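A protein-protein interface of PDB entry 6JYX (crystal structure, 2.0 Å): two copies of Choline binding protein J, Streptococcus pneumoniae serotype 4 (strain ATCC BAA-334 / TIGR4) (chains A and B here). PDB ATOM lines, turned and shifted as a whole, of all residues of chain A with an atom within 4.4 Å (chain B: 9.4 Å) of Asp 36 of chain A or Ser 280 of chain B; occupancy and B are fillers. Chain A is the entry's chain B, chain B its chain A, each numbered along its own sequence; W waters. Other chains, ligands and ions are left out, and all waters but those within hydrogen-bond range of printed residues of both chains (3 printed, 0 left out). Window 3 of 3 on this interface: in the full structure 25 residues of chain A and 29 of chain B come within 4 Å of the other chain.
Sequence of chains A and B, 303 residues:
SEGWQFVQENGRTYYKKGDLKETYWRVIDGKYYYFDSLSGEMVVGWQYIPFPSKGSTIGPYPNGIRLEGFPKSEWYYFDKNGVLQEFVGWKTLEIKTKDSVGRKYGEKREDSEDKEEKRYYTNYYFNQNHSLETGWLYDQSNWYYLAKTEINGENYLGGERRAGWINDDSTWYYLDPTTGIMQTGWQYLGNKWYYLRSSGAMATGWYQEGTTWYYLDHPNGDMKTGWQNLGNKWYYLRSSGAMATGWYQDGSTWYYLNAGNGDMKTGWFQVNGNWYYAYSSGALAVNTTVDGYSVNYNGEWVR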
ATOM      1  N   THR A  23       7.668  -6.642   6.565  1.00  0.00           N
ATOM      2  CA  THR A  23       6.970  -6.653   7.852  1.00  0.00           C
ATOM      3  C   THR A  23       5.529  -7.153   7.696  1.00  0.00           C
ATOM      4  O   THR A  23       4.934  -7.066   6.620  1.00  0.00           O
ATOM      5  CB  THR A  23       7.010  -5.260   8.531  1.00  0.00           C
ATOM      6  OG1 THR A  23       6.459  -4.287   7.632  1.00  0.00           O
ATOM      7  CG2 THR A  23       8.451  -4.877   8.869  1.00  0.00           C
ATOM      8  N   TYR A  34       5.115 -14.524   8.588  1.00  0.00           N
ATOM      9  CA  TYR A  34       4.829 -13.265   9.215  1.00  0.00           C
ATOM     10  C   TYR A  34       6.082 -12.794   9.942  1.00  0.00           C
ATOM     11  O   TYR A  34       6.776 -13.577  10.641  1.00  0.00           O
ATOM     12  CB  TYR A  34       3.590 -13.399  10.130  1.00  0.00           C
ATOM     13  CG  TYR A  34       3.208 -12.127  10.888  1.00  0.00           C
ATOM     14  CD1 TYR A  34       2.118 -11.358  10.479  1.00  0.00           C
ATOM     15  CD2 TYR A  34       3.894 -11.740  12.029  1.00  0.00           C
ATOM     16  CE1 TYR A  34       1.735 -10.198  11.189  1.00  0.00           C
ATOM     17  CE2 TYR A  34       3.516 -10.570  12.754  1.00  0.00           C
ATOM     18  CZ  TYR A  34       2.421  -9.838  12.321  1.00  0.00           C
ATOM     19  OH  TYR A  34       2.041  -8.693  12.989  1.00  0.00           O
ATOM     20  N   PHE A  35       6.356 -11.510   9.754  1.00  0.00           N
ATOM     21  CA  PHE A  35       7.548 -10.836  10.247  1.00  0.00           C
ATOM     22  C   PHE A  35       7.179  -9.673  11.176  1.00  0.00           C
ATOM     23  O   PHE A  35       6.288  -8.868  10.874  1.00  0.00           O
ATOM     24  CB  PHE A  35       8.342 -10.333   9.021  1.00  0.00           C
ATOM     25  CG  PHE A  35       8.664 -11.440   8.038  1.00  0.00           C
ATOM     26  CD1 PHE A  35       7.810 -11.740   6.976  1.00  0.00           C
ATOM     27  CD2 PHE A  35       9.791 -12.231   8.230  1.00  0.00           C
ATOM     28  CE1 PHE A  35       8.101 -12.794   6.099  1.00  0.00           C
ATOM     29  CE2 PHE A  35      10.082 -13.274   7.361  1.00  0.00           C
ATOM     30  CZ  PHE A  35       9.229 -13.562   6.295  1.00  0.00           C
ATOM     31  N   ASP A  36       7.885  -9.572  12.292  1.00  0.00           N
ATOM     32  CA  ASP A  36       7.528  -8.586  13.322  1.00  0.00           C
ATOM     33  C   ASP A  36       7.402  -7.179  12.738  1.00  0.00           C
ATOM     34  O   ASP A  36       8.241  -6.775  11.906  1.00  0.00           O
ATOM     35  CB  ASP A  36       8.564  -8.588  14.421  1.00  0.00           C
ATOM     36  CG  ASP A  36       8.216  -7.592  15.523  1.00  0.00           C
ATOM     37  OD1 ASP A  36       7.349  -7.925  16.368  1.00  0.00           O
ATOM     38  OD2 ASP A  36       8.774  -6.470  15.502  1.00  0.00           O
ATOM     39  N   SER A  37       6.347  -6.452  13.138  1.00  0.00           N
ATOM     40  CA  SER A  37       6.026  -5.144  12.529  1.00  0.00           C
ATOM     41  C   SER A  37       7.165  -4.121  12.644  1.00  0.00           C
ATOM     42  O   SER A  37       7.300  -3.261  11.796  1.00  0.00           O
ATOM     43  CB  SER A  37       4.779  -4.528  13.170  1.00  0.00           C
ATOM     44  OG  SER A  37       4.980  -4.304  14.546  1.00  0.00           O
ATOM     45  N   LEU A  38       7.965  -4.218  13.691  1.00  0.00           N
ATOM     46  CA  LEU A  38       9.035  -3.255  13.910  1.00  0.00           C
ATOM     47  C   LEU A  38      10.379  -3.769  13.419  1.00  0.00           C
ATOM     48  O   LEU A  38      11.071  -3.070  12.698  1.00  0.00           O
ATOM     49  CB  LEU A  38       9.147  -2.869  15.390  1.00  0.00           C
ATOM     50  CG  LEU A  38       7.920  -2.204  16.039  1.00  0.00           C
ATOM     51  CD1 LEU A  38       8.199  -1.973  17.507  1.00  0.00           C
ATOM     52  CD2 LEU A  38       7.548  -0.893  15.357  1.00  0.00           C
ATOM     53  N   SER A  39      10.748  -4.991  13.808  1.00  0.00           N
ATOM     54  CA  SER A  39      12.093  -5.509  13.522  1.00  0.00           C
ATOM     55  C   SER A  39      12.223  -6.373  12.245  1.00  0.00           C
ATOM     56  O   SER A  39      13.327  -6.610  11.765  1.00  0.00           O
ATOM     57  CB  SER A  39      12.544  -6.334  14.713  1.00  0.00           C
ATOM     58  OG  SER A  39      11.745  -7.499  14.783  1.00  0.00           O
ATOM     59  N   GLY A  40      11.111  -6.888  11.734  1.00  0.00           N
ATOM     60  CA  GLY A  40      11.140  -7.852  10.639  1.00  0.00           C
ATOM     61  C   GLY A  40      11.531  -9.267  11.048  1.00  0.00           C
ATOM     62  O   GLY A  40      11.671 -10.141  10.183  1.00  0.00           O
ATOM     63  N   GLU A  41      11.733  -9.519  12.338  1.00  0.00           N
ATOM     64  CA  GLU A  41      12.085 -10.889  12.752  1.00  0.00           C
ATOM     65  C   GLU A  41      10.899 -11.801  12.429  1.00  0.00           C
ATOM     66  O   GLU A  41       9.751 -11.487  12.766  1.00  0.00           O
ATOM     67  CB  GLU A  41      12.468 -10.980  14.243  1.00  0.00           C
ATOM     68  CG  GLU A  41      13.717 -10.167  14.625  1.00  0.00           C
ATOM     69  CD  GLU A  41      13.960 -10.100  16.149  1.00  0.00           C
ATOM     70  OE1 GLU A  41      13.696 -11.099  16.865  1.00  0.00           O
ATOM     71  OE2 GLU A  41      14.446  -9.055  16.625  1.00  0.00           O
ATOM     72  N   LYS A 104      10.215 -15.487  18.296  1.00  0.00           N
ATOM     73  CA  LYS A 104      10.741 -15.273  16.949  1.00  0.00           C
ATOM     74  C   LYS A 104      11.703 -16.411  16.648  1.00  0.00           C
ATOM     75  O   LYS A 104      12.365 -16.942  17.558  1.00  0.00           O
ATOM     76  CB  LYS A 104      11.503 -13.937  16.845  1.00  0.00           C
ATOM     77  CG  LYS A 104      10.750 -12.721  17.424  1.00  0.00           C
ATOM     78  CD  LYS A 104       9.495 -12.439  16.584  1.00  0.00           C
ATOM     79  CE  LYS A 104       8.786 -11.185  17.061  1.00  0.00           C
ATOM     80  NZ  LYS A 104       8.400 -11.290  18.484  1.00  0.00           N
ATOM     81  N   TRP B 227       8.344 -10.346  34.853  1.00  0.00           N
ATOM     82  CA  TRP B 227       7.947  -9.743  33.578  1.00  0.00           C
ATOM     83  C   TRP B 227       6.444  -9.740  33.420  1.00  0.00           C
ATOM     84  O   TRP B 227       5.793 -10.765  33.628  1.00  0.00           O
ATOM     85  CB  TRP B 227       8.575 -10.528  32.438  1.00  0.00           C
ATOM     86  CG  TRP B 227      10.044 -10.389  32.398  1.00  0.00           C
ATOM     87  CD1 TRP B 227      10.981 -11.283  32.847  1.00  0.00           C
ATOM     88  CD2 TRP B 227      10.762  -9.266  31.889  1.00  0.00           C
ATOM     89  NE1 TRP B 227      12.244 -10.771  32.643  1.00  0.00           N
ATOM     90  CE2 TRP B 227      12.135  -9.538  32.051  1.00  0.00           C
ATOM     91  CE3 TRP B 227      10.375  -8.056  31.309  1.00  0.00           C
ATOM     92  CZ2 TRP B 227      13.137  -8.639  31.643  1.00  0.00           C
ATOM     93  CZ3 TRP B 227      11.387  -7.149  30.901  1.00  0.00           C
ATOM     94  CH2 TRP B 227      12.742  -7.464  31.069  1.00  0.00           C
ATOM     95  N   ASN B 229       3.347  -8.276  30.689  1.00  0.00           N
ATOM     96  CA  ASN B 229       2.953  -7.568  29.494  1.00  0.00           C
ATOM     97  C   ASN B 229       1.692  -6.797  29.784  1.00  0.00           C
ATOM     98  O   ASN B 229       0.610  -7.398  29.957  1.00  0.00           O
ATOM     99  CB  ASN B 229       2.755  -8.521  28.308  1.00  0.00           C
ATOM    100  CG  ASN B 229       2.714  -7.784  26.985  1.00  0.00           C
ATOM    101  OD1 ASN B 229       1.884  -6.892  26.772  1.00  0.00           O
ATOM    102  ND2 ASN B 229       3.622  -8.130  26.100  1.00  0.00           N
ATOM    103  N   ASN B 232       0.433  -3.884  26.030  1.00  0.00           N
ATOM    104  CA  ASN B 232       1.336  -4.185  24.911  1.00  0.00           C
ATOM    105  C   ASN B 232       2.794  -3.727  25.092  1.00  0.00           C
ATOM    106  O   ASN B 232       3.554  -3.676  24.122  1.00  0.00           O
ATOM    107  CB  ASN B 232       0.737  -3.679  23.581  1.00  0.00           C
ATOM    108  CG  ASN B 232      -0.617  -4.319  23.268  1.00  0.00           C
ATOM    109  OD1 ASN B 232      -0.849  -5.510  23.538  1.00  0.00           O
ATOM    110  ND2 ASN B 232      -1.519  -3.528  22.697  1.00  0.00           N
ATOM    111  N   TRP B 234       6.314  -4.380  27.807  1.00  0.00           N
ATOM    112  CA  TRP B 234       6.880  -5.243  28.805  1.00  0.00           C
ATOM    113  C   TRP B 234       7.433  -4.433  29.986  1.00  0.00           C
ATOM    114  O   TRP B 234       8.122  -3.426  29.797  1.00  0.00           O
ATOM    115  CB  TRP B 234       7.997  -6.082  28.207  1.00  0.00           C
ATOM    116  CG  TRP B 234       7.509  -7.284  27.443  1.00  0.00           C
ATOM    117  CD1 TRP B 234       7.465  -7.434  26.079  1.00  0.00           C
ATOM    118  CD2 TRP B 234       6.985  -8.511  27.999  1.00  0.00           C
ATOM    119  NE1 TRP B 234       6.967  -8.683  25.755  1.00  0.00           N
ATOM    120  CE2 TRP B 234       6.654  -9.357  26.909  1.00  0.00           C
ATOM    121  CE3 TRP B 234       6.765  -8.972  29.304  1.00  0.00           C
ATOM    122  CZ2 TRP B 234       6.106 -10.634  27.088  1.00  0.00           C
ATOM    123  CZ3 TRP B 234       6.227 -10.253  29.487  1.00  0.00           C
ATOM    124  CH2 TRP B 234       5.904 -11.068  28.374  1.00  0.00           C
ATOM    125  N   TYR B 255      18.617  -6.087  29.469  1.00  0.00           N
ATOM    126  CA  TYR B 255      17.414  -5.420  28.991  1.00  0.00           C
ATOM    127  C   TYR B 255      17.465  -3.983  29.406  1.00  0.00           C
ATOM    128  O   TYR B 255      18.059  -3.666  30.431  1.00  0.00           O
ATOM    129  CB  TYR B 255      16.157  -6.067  29.594  1.00  0.00           C
ATOM    130  CG  TYR B 255      16.054  -7.506  29.220  1.00  0.00           C
ATOM    131  CD1 TYR B 255      16.673  -8.496  29.997  1.00  0.00           C
ATOM    132  CD2 TYR B 255      15.372  -7.885  28.064  1.00  0.00           C
ATOM    133  CE1 TYR B 255      16.594  -9.828  29.645  1.00  0.00           C
ATOM    134  CE2 TYR B 255      15.296  -9.221  27.683  1.00  0.00           C
ATOM    135  CZ  TYR B 255      15.896 -10.186  28.491  1.00  0.00           C
ATOM    136  OH  TYR B 255      15.829 -11.499  28.115  1.00  0.00           O
ATOM    137  N   MET B 264       9.990  -1.718  28.514  1.00  0.00           N
ATOM    138  CA  MET B 264      11.182  -2.315  27.931  1.00  0.00           C
ATOM    139  C   MET B 264      11.344  -1.739  26.522  1.00  0.00           C
ATOM    140  O   MET B 264      10.356  -1.564  25.794  1.00  0.00           O
ATOM    141  CB  MET B 264      11.036  -3.839  27.892  1.00  0.00           C
ATOM    142  CG  MET B 264      12.252  -4.641  27.401  1.00  0.00           C
ATOM    143  SD  MET B 264      11.862  -6.382  27.031  1.00  0.00           S
ATOM    144  CE  MET B 264      10.920  -6.177  25.502  1.00  0.00           C
ATOM    145  N   LYS B 265      12.583  -1.389  26.180  1.00  0.00           N
ATOM    146  CA  LYS B 265      12.898  -0.832  24.863  1.00  0.00           C
ATOM    147  C   LYS B 265      13.250  -1.938  23.911  1.00  0.00           C
ATOM    148  O   LYS B 265      13.903  -2.913  24.300  1.00  0.00           O
ATOM    149  CB  LYS B 265      14.098   0.137  24.978  1.00  0.00           C
ATOM    150  CG  LYS B 265      13.719   1.513  25.452  1.00  0.00           C
ATOM    151  CD  LYS B 265      13.367   2.352  24.254  1.00  0.00           C
ATOM    152  CE  LYS B 265      12.387   3.434  24.606  1.00  0.00           C
ATOM    153  NZ  LYS B 265      11.678   3.884  23.358  1.00  0.00           N
ATOM    154  N   THR B 266      12.820  -1.810  22.663  1.00  0.00           N
ATOM    155  CA  THR B 266      13.368  -2.655  21.588  1.00  0.00           C
ATOM    156  C   THR B 266      13.790  -1.758  20.419  1.00  0.00           C
ATOM    157  O   THR B 266      13.388  -0.590  20.351  1.00  0.00           O
ATOM    158  CB  THR B 266      12.359  -3.739  21.068  1.00  0.00           C
ATOM    159  OG1 THR B 266      11.349  -3.118  20.289  1.00  0.00           O
ATOM    160  CG2 THR B 266      11.681  -4.519  22.218  1.00  0.00           C
ATOM    161  N   GLY B 267      14.556  -2.316  19.495  1.00  0.00           N
ATOM    162  CA  GLY B 267      15.136  -1.533  18.396  1.00  0.00           C
ATOM    163  C   GLY B 267      16.353  -0.730  18.859  1.00  0.00           C
ATOM    164  O   GLY B 267      17.041  -1.118  19.835  1.00  0.00           O
ATOM    165  N   TRP B 268      16.636   0.358  18.126  1.00  0.00           N
ATOM    166  CA  TRP B 268      17.733   1.290  18.441  1.00  0.00           C
ATOM    167  C   TRP B 268      17.277   2.290  19.486  1.00  0.00           C
ATOM    168  O   TRP B 268      16.197   2.899  19.380  1.00  0.00           O
ATOM    169  CB  TRP B 268      18.249   2.046  17.182  1.00  0.00           C
ATOM    170  CG  TRP B 268      19.056   1.172  16.283  1.00  0.00           C
ATOM    171  CD1 TRP B 268      18.652   0.619  15.096  1.00  0.00           C
ATOM    172  CD2 TRP B 268      20.384   0.691  16.512  1.00  0.00           C
ATOM    173  NE1 TRP B 268      19.639  -0.157  14.583  1.00  0.00           N
ATOM    174  CE2 TRP B 268      20.718  -0.132  15.426  1.00  0.00           C
ATOM    175  CE3 TRP B 268      21.326   0.878  17.533  1.00  0.00           C
ATOM    176  CZ2 TRP B 268      21.958  -0.769  15.320  1.00  0.00           C
ATOM    177  CZ3 TRP B 268      22.558   0.240  17.427  1.00  0.00           C
ATOM    178  CH2 TRP B 268      22.860  -0.569  16.325  1.00  0.00           C
ATOM    179  N   TYR B 277      21.226  -1.588  20.633  1.00  0.00           N
ATOM    180  CA  TYR B 277      20.155  -2.251  19.887  1.00  0.00           C
ATOM    181  C   TYR B 277      19.581  -3.409  20.681  1.00  0.00           C
ATOM    182  O   TYR B 277      20.336  -4.247  21.167  1.00  0.00           O
ATOM    183  CB  TYR B 277      20.660  -2.780  18.548  1.00  0.00           C
ATOM    184  CG  TYR B 277      19.561  -3.435  17.730  1.00  0.00           C
ATOM    185  CD1 TYR B 277      18.658  -2.658  17.026  1.00  0.00           C
ATOM    186  CD2 TYR B 277      19.431  -4.819  17.663  1.00  0.00           C
ATOM    187  CE1 TYR B 277      17.646  -3.228  16.266  1.00  0.00           C
ATOM    188  CE2 TYR B 277      18.390  -5.417  16.896  1.00  0.00           C
ATOM    189  CZ  TYR B 277      17.515  -4.597  16.204  1.00  0.00           C
ATOM    190  OH  TYR B 277      16.502  -5.108  15.445  1.00  0.00           O
ATOM    191  N   ALA B 278      18.255  -3.457  20.807  1.00  0.00           N
ATOM    192  CA  ALA B 278      17.630  -4.633  21.421  1.00  0.00           C
ATOM    193  C   ALA B 278      16.772  -5.347  20.399  1.00  0.00           C
ATOM    194  O   ALA B 278      16.041  -4.702  19.639  1.00  0.00           O
ATOM    195  CB  ALA B 278      16.819  -4.252  22.638  1.00  0.00           C
ATOM    196  N   TYR B 279      16.882  -6.663  20.366  1.00  0.00           N
ATOM    197  CA  TYR B 279      16.036  -7.492  19.482  1.00  0.00           C
ATOM    198  C   TYR B 279      14.566  -7.402  19.927  1.00  0.00           C
ATOM    199  O   TYR B 279      14.256  -6.774  20.945  1.00  0.00           O
ATOM    200  CB  TYR B 279      16.496  -8.951  19.529  1.00  0.00           C
ATOM    201  CG  TYR B 279      17.977  -9.181  19.222  1.00  0.00           C
ATOM    202  CD1 TYR B 279      18.853  -9.633  20.209  1.00  0.00           C
ATOM    203  CD2 TYR B 279      18.485  -8.955  17.945  1.00  0.00           C
ATOM    204  CE1 TYR B 279      20.214  -9.846  19.930  1.00  0.00           C
ATOM    205  CE2 TYR B 279      19.822  -9.144  17.662  1.00  0.00           C
ATOM    206  CZ  TYR B 279      20.685  -9.597  18.653  1.00  0.00           C
ATOM    207  OH  TYR B 279      22.013  -9.819  18.349  1.00  0.00           O
ATOM    208  N   SER B 280      13.656  -8.022  19.178  1.00  0.00           N
ATOM    209  CA  SER B 280      12.241  -8.002  19.576  1.00  0.00           C
ATOM    210  C   SER B 280      12.033  -8.565  21.001  1.00  0.00           C
ATOM    211  O   SER B 280      11.113  -8.157  21.689  1.00  0.00           O
ATOM    212  CB  SER B 280      11.364  -8.783  18.591  1.00  0.00           C
ATOM    213  OG  SER B 280      11.259  -8.129  17.329  1.00  0.00           O
ATOM    214  N   SER B 281      12.869  -9.514  21.420  1.00  0.00           N
ATOM    215  CA  SER B 281      12.757 -10.064  22.780  1.00  0.00           C
ATOM    216  C   SER B 281      13.145  -9.053  23.852  1.00  0.00           C
ATOM    217  O   SER B 281      12.958  -9.300  25.055  1.00  0.00           O
ATOM    218  CB  SER B 281      13.662 -11.278  22.919  1.00  0.00           C
ATOM    219  OG  SER B 281      15.025 -10.886  22.803  1.00  0.00           O
ATOM    220  N   GLY B 282      13.723  -7.932  23.435  1.00  0.00           N
ATOM    221  CA  GLY B 282      14.250  -6.961  24.381  1.00  0.00           C
ATOM    222  C   GLY B 282      15.701  -7.192  24.745  1.00  0.00           C
ATOM    223  O   GLY B 282      16.321  -6.339  25.412  1.00  0.00           O
ATOM    224  N   ALA B 283      16.247  -8.340  24.357  1.00  0.00           N
ATOM    225  CA  ALA B 283      17.635  -8.657  24.672  1.00  0.00           C
ATOM    226  C   ALA B 283      18.601  -7.732  23.912  1.00  0.00           C
ATOM    227  O   ALA B 283      18.472  -7.532  22.697  1.00  0.00           O
ATOM    228  CB  ALA B 283      17.931 -10.087  24.322  1.00  0.00           C
ATOM    229  N   LEU B 284      19.565  -7.187  24.642  1.00  0.00           N
ATOM    230  CA  LEU B 284      20.601  -6.312  24.074  1.00  0.00           C
ATOM    231  C   LEU B 284      21.544  -7.068  23.116  1.00  0.00           C
ATOM    232  O   LEU B 284      22.072  -8.125  23.455  1.00  0.00           O
ATOM    233  CB  LEU B 284      21.392  -5.645  25.216  1.00  0.00           C
ATOM    234  CG  LEU B 284      22.563  -4.741  24.791  1.00  0.00           C
ATOM    235  CD1 LEU B 284      21.999  -3.442  24.231  1.00  0.00           C
ATOM    236  CD2 LEU B 284      23.485  -4.460  25.984  1.00  0.00           C
ATOM    237  N   ALA B 285      21.734  -6.538  21.908  1.00  0.00           N
ATOM    238  CA  ALA B 285      22.709  -7.114  20.969  1.00  0.00           C
ATOM    239  C   ALA B 285      24.113  -6.728  21.457  1.00  0.00           C
ATOM    240  O   ALA B 285      24.379  -5.542  21.698  1.00  0.00           O
ATOM    241  CB  ALA B 285      22.471  -6.591  19.550  1.00  0.00           C
ATOM    242  N   VAL B 290      24.629  -5.582  13.590  1.00  0.00           N
ATOM    243  CA  VAL B 290      23.197  -5.380  13.425  1.00  0.00           C
ATOM    244  C   VAL B 290      23.010  -4.262  12.407  1.00  0.00           C
ATOM    245  O   VAL B 290      23.469  -3.142  12.643  1.00  0.00           O
ATOM    246  CB  VAL B 290      22.524  -4.903  14.746  1.00  0.00           C
ATOM    247  CG1 VAL B 290      21.036  -4.676  14.527  1.00  0.00           C
ATOM    248  CG2 VAL B 290      22.771  -5.886  15.885  1.00  0.00           C
HETATM  249  O   HOH W   1      16.105  -7.854  14.952  1.00  0.00           O
HETATM  250  O   HOH W   2       9.879  -5.802  17.746  1.00  0.00           O
HETATM  251  O   HOH W   3      13.902 -11.485  19.379  1.00  0.00           O
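N of Ser 280 of chain B is in hydrogen-bond range of OE2 of Glu 41 of chain A, 2.9 Å away.
OG of Ser 39 of chain A sits at hydrogen-bond distance from OG of Ser 280 of chain B.
Of chain B, only Ser 280 (3.5 Å) comes within 4 Å of Asp 36 of chain A.
Ser 39 of chain A touches one residue of chain B.
No residue of chain B comes within 4 Å of Gly 40 of chain A.
Printed residues of chain B within 4 Å of Lys 104 of chain A: Ser 280.
Printed residues of chain A within 4 Å of Tyr 279 of chain B: Glu 41.
Of chain A, only Asp 36, Ser 39, Glu 41 and Lys 104 come within 4 Å of Ser 280 of chain B.
Ala 283 of chain B touches none of the printed residues of chain A.
The nearest residue of chain B that does not touch Asp 36 of chain A is Thr 266 of chain B (6.4 Å).
The nearest printed residue of chain A that does not touch Ser 280 of chain B is Gly 40 of chain A (5.7 Å).
Hydrophobic or aromatic side chains of chain B within 4 Å of the printed part of chain A: Tyr 279.
Among the printed residues, 5 pairs touch across the chains.
Among the printed residues, no Asp or Glu carboxylate lies within 4 Å of a Lys or Arg side-chain nitrogen of the other chain.
OG of Ser 39 of chain A sits at hydrogen-bond distance from N of Glu 41 of chain A, at 3.2 Å.
The side-chain carboxylate (OD2) of Asp 36 of chain A sits at hydrogen-bond distance from the backbone NH (N) of Ser 39 of chain A (3.0 Å).
OD2 of Asp 36 of chain A sits at hydrogen-bond distance from N of Leu 38 of chain A, at 3.0 Å.
The backbone NH of Asp 36 of chain A is in hydrogen-bond range of the backbone carbonyl oxygen of Glu 41 of chain A (2.7 Å).
Asp 36 of chain A touches Ser 280 of chain B.
OE2 of Glu 41 of chain A touches CB of Tyr 279 of chain B, 3.6 Å away.
Lys 104 of chain A touches Ser 280 of chain B (CE to CB, 3.8 Å).
No position is printed for both chains.
Of the 5 pairs that touch across the chains among the printed residues, none has its exchanged pair printed and touching as well.
Water W3 lies within hydrogen-bond range of OE1 of Glu 41 of chain A (2.6 Å), N of Ser 281 of chain B (3.0 Å) and N of Ser 280 of chain B (3.5 Å).
Water W2 bridges the side-chain carboxylate (OD2) of Asp 36 of chain A (2.6 Å) and the side-chain hydroxyl (OG) of Ser 280 of chain B (2.7 Å).
Water W1 lies within hydrogen-bond range of OE2 of Glu 41 of chain A (2.6 Å) and OH of Tyr 277 of chain B (2.8 Å).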
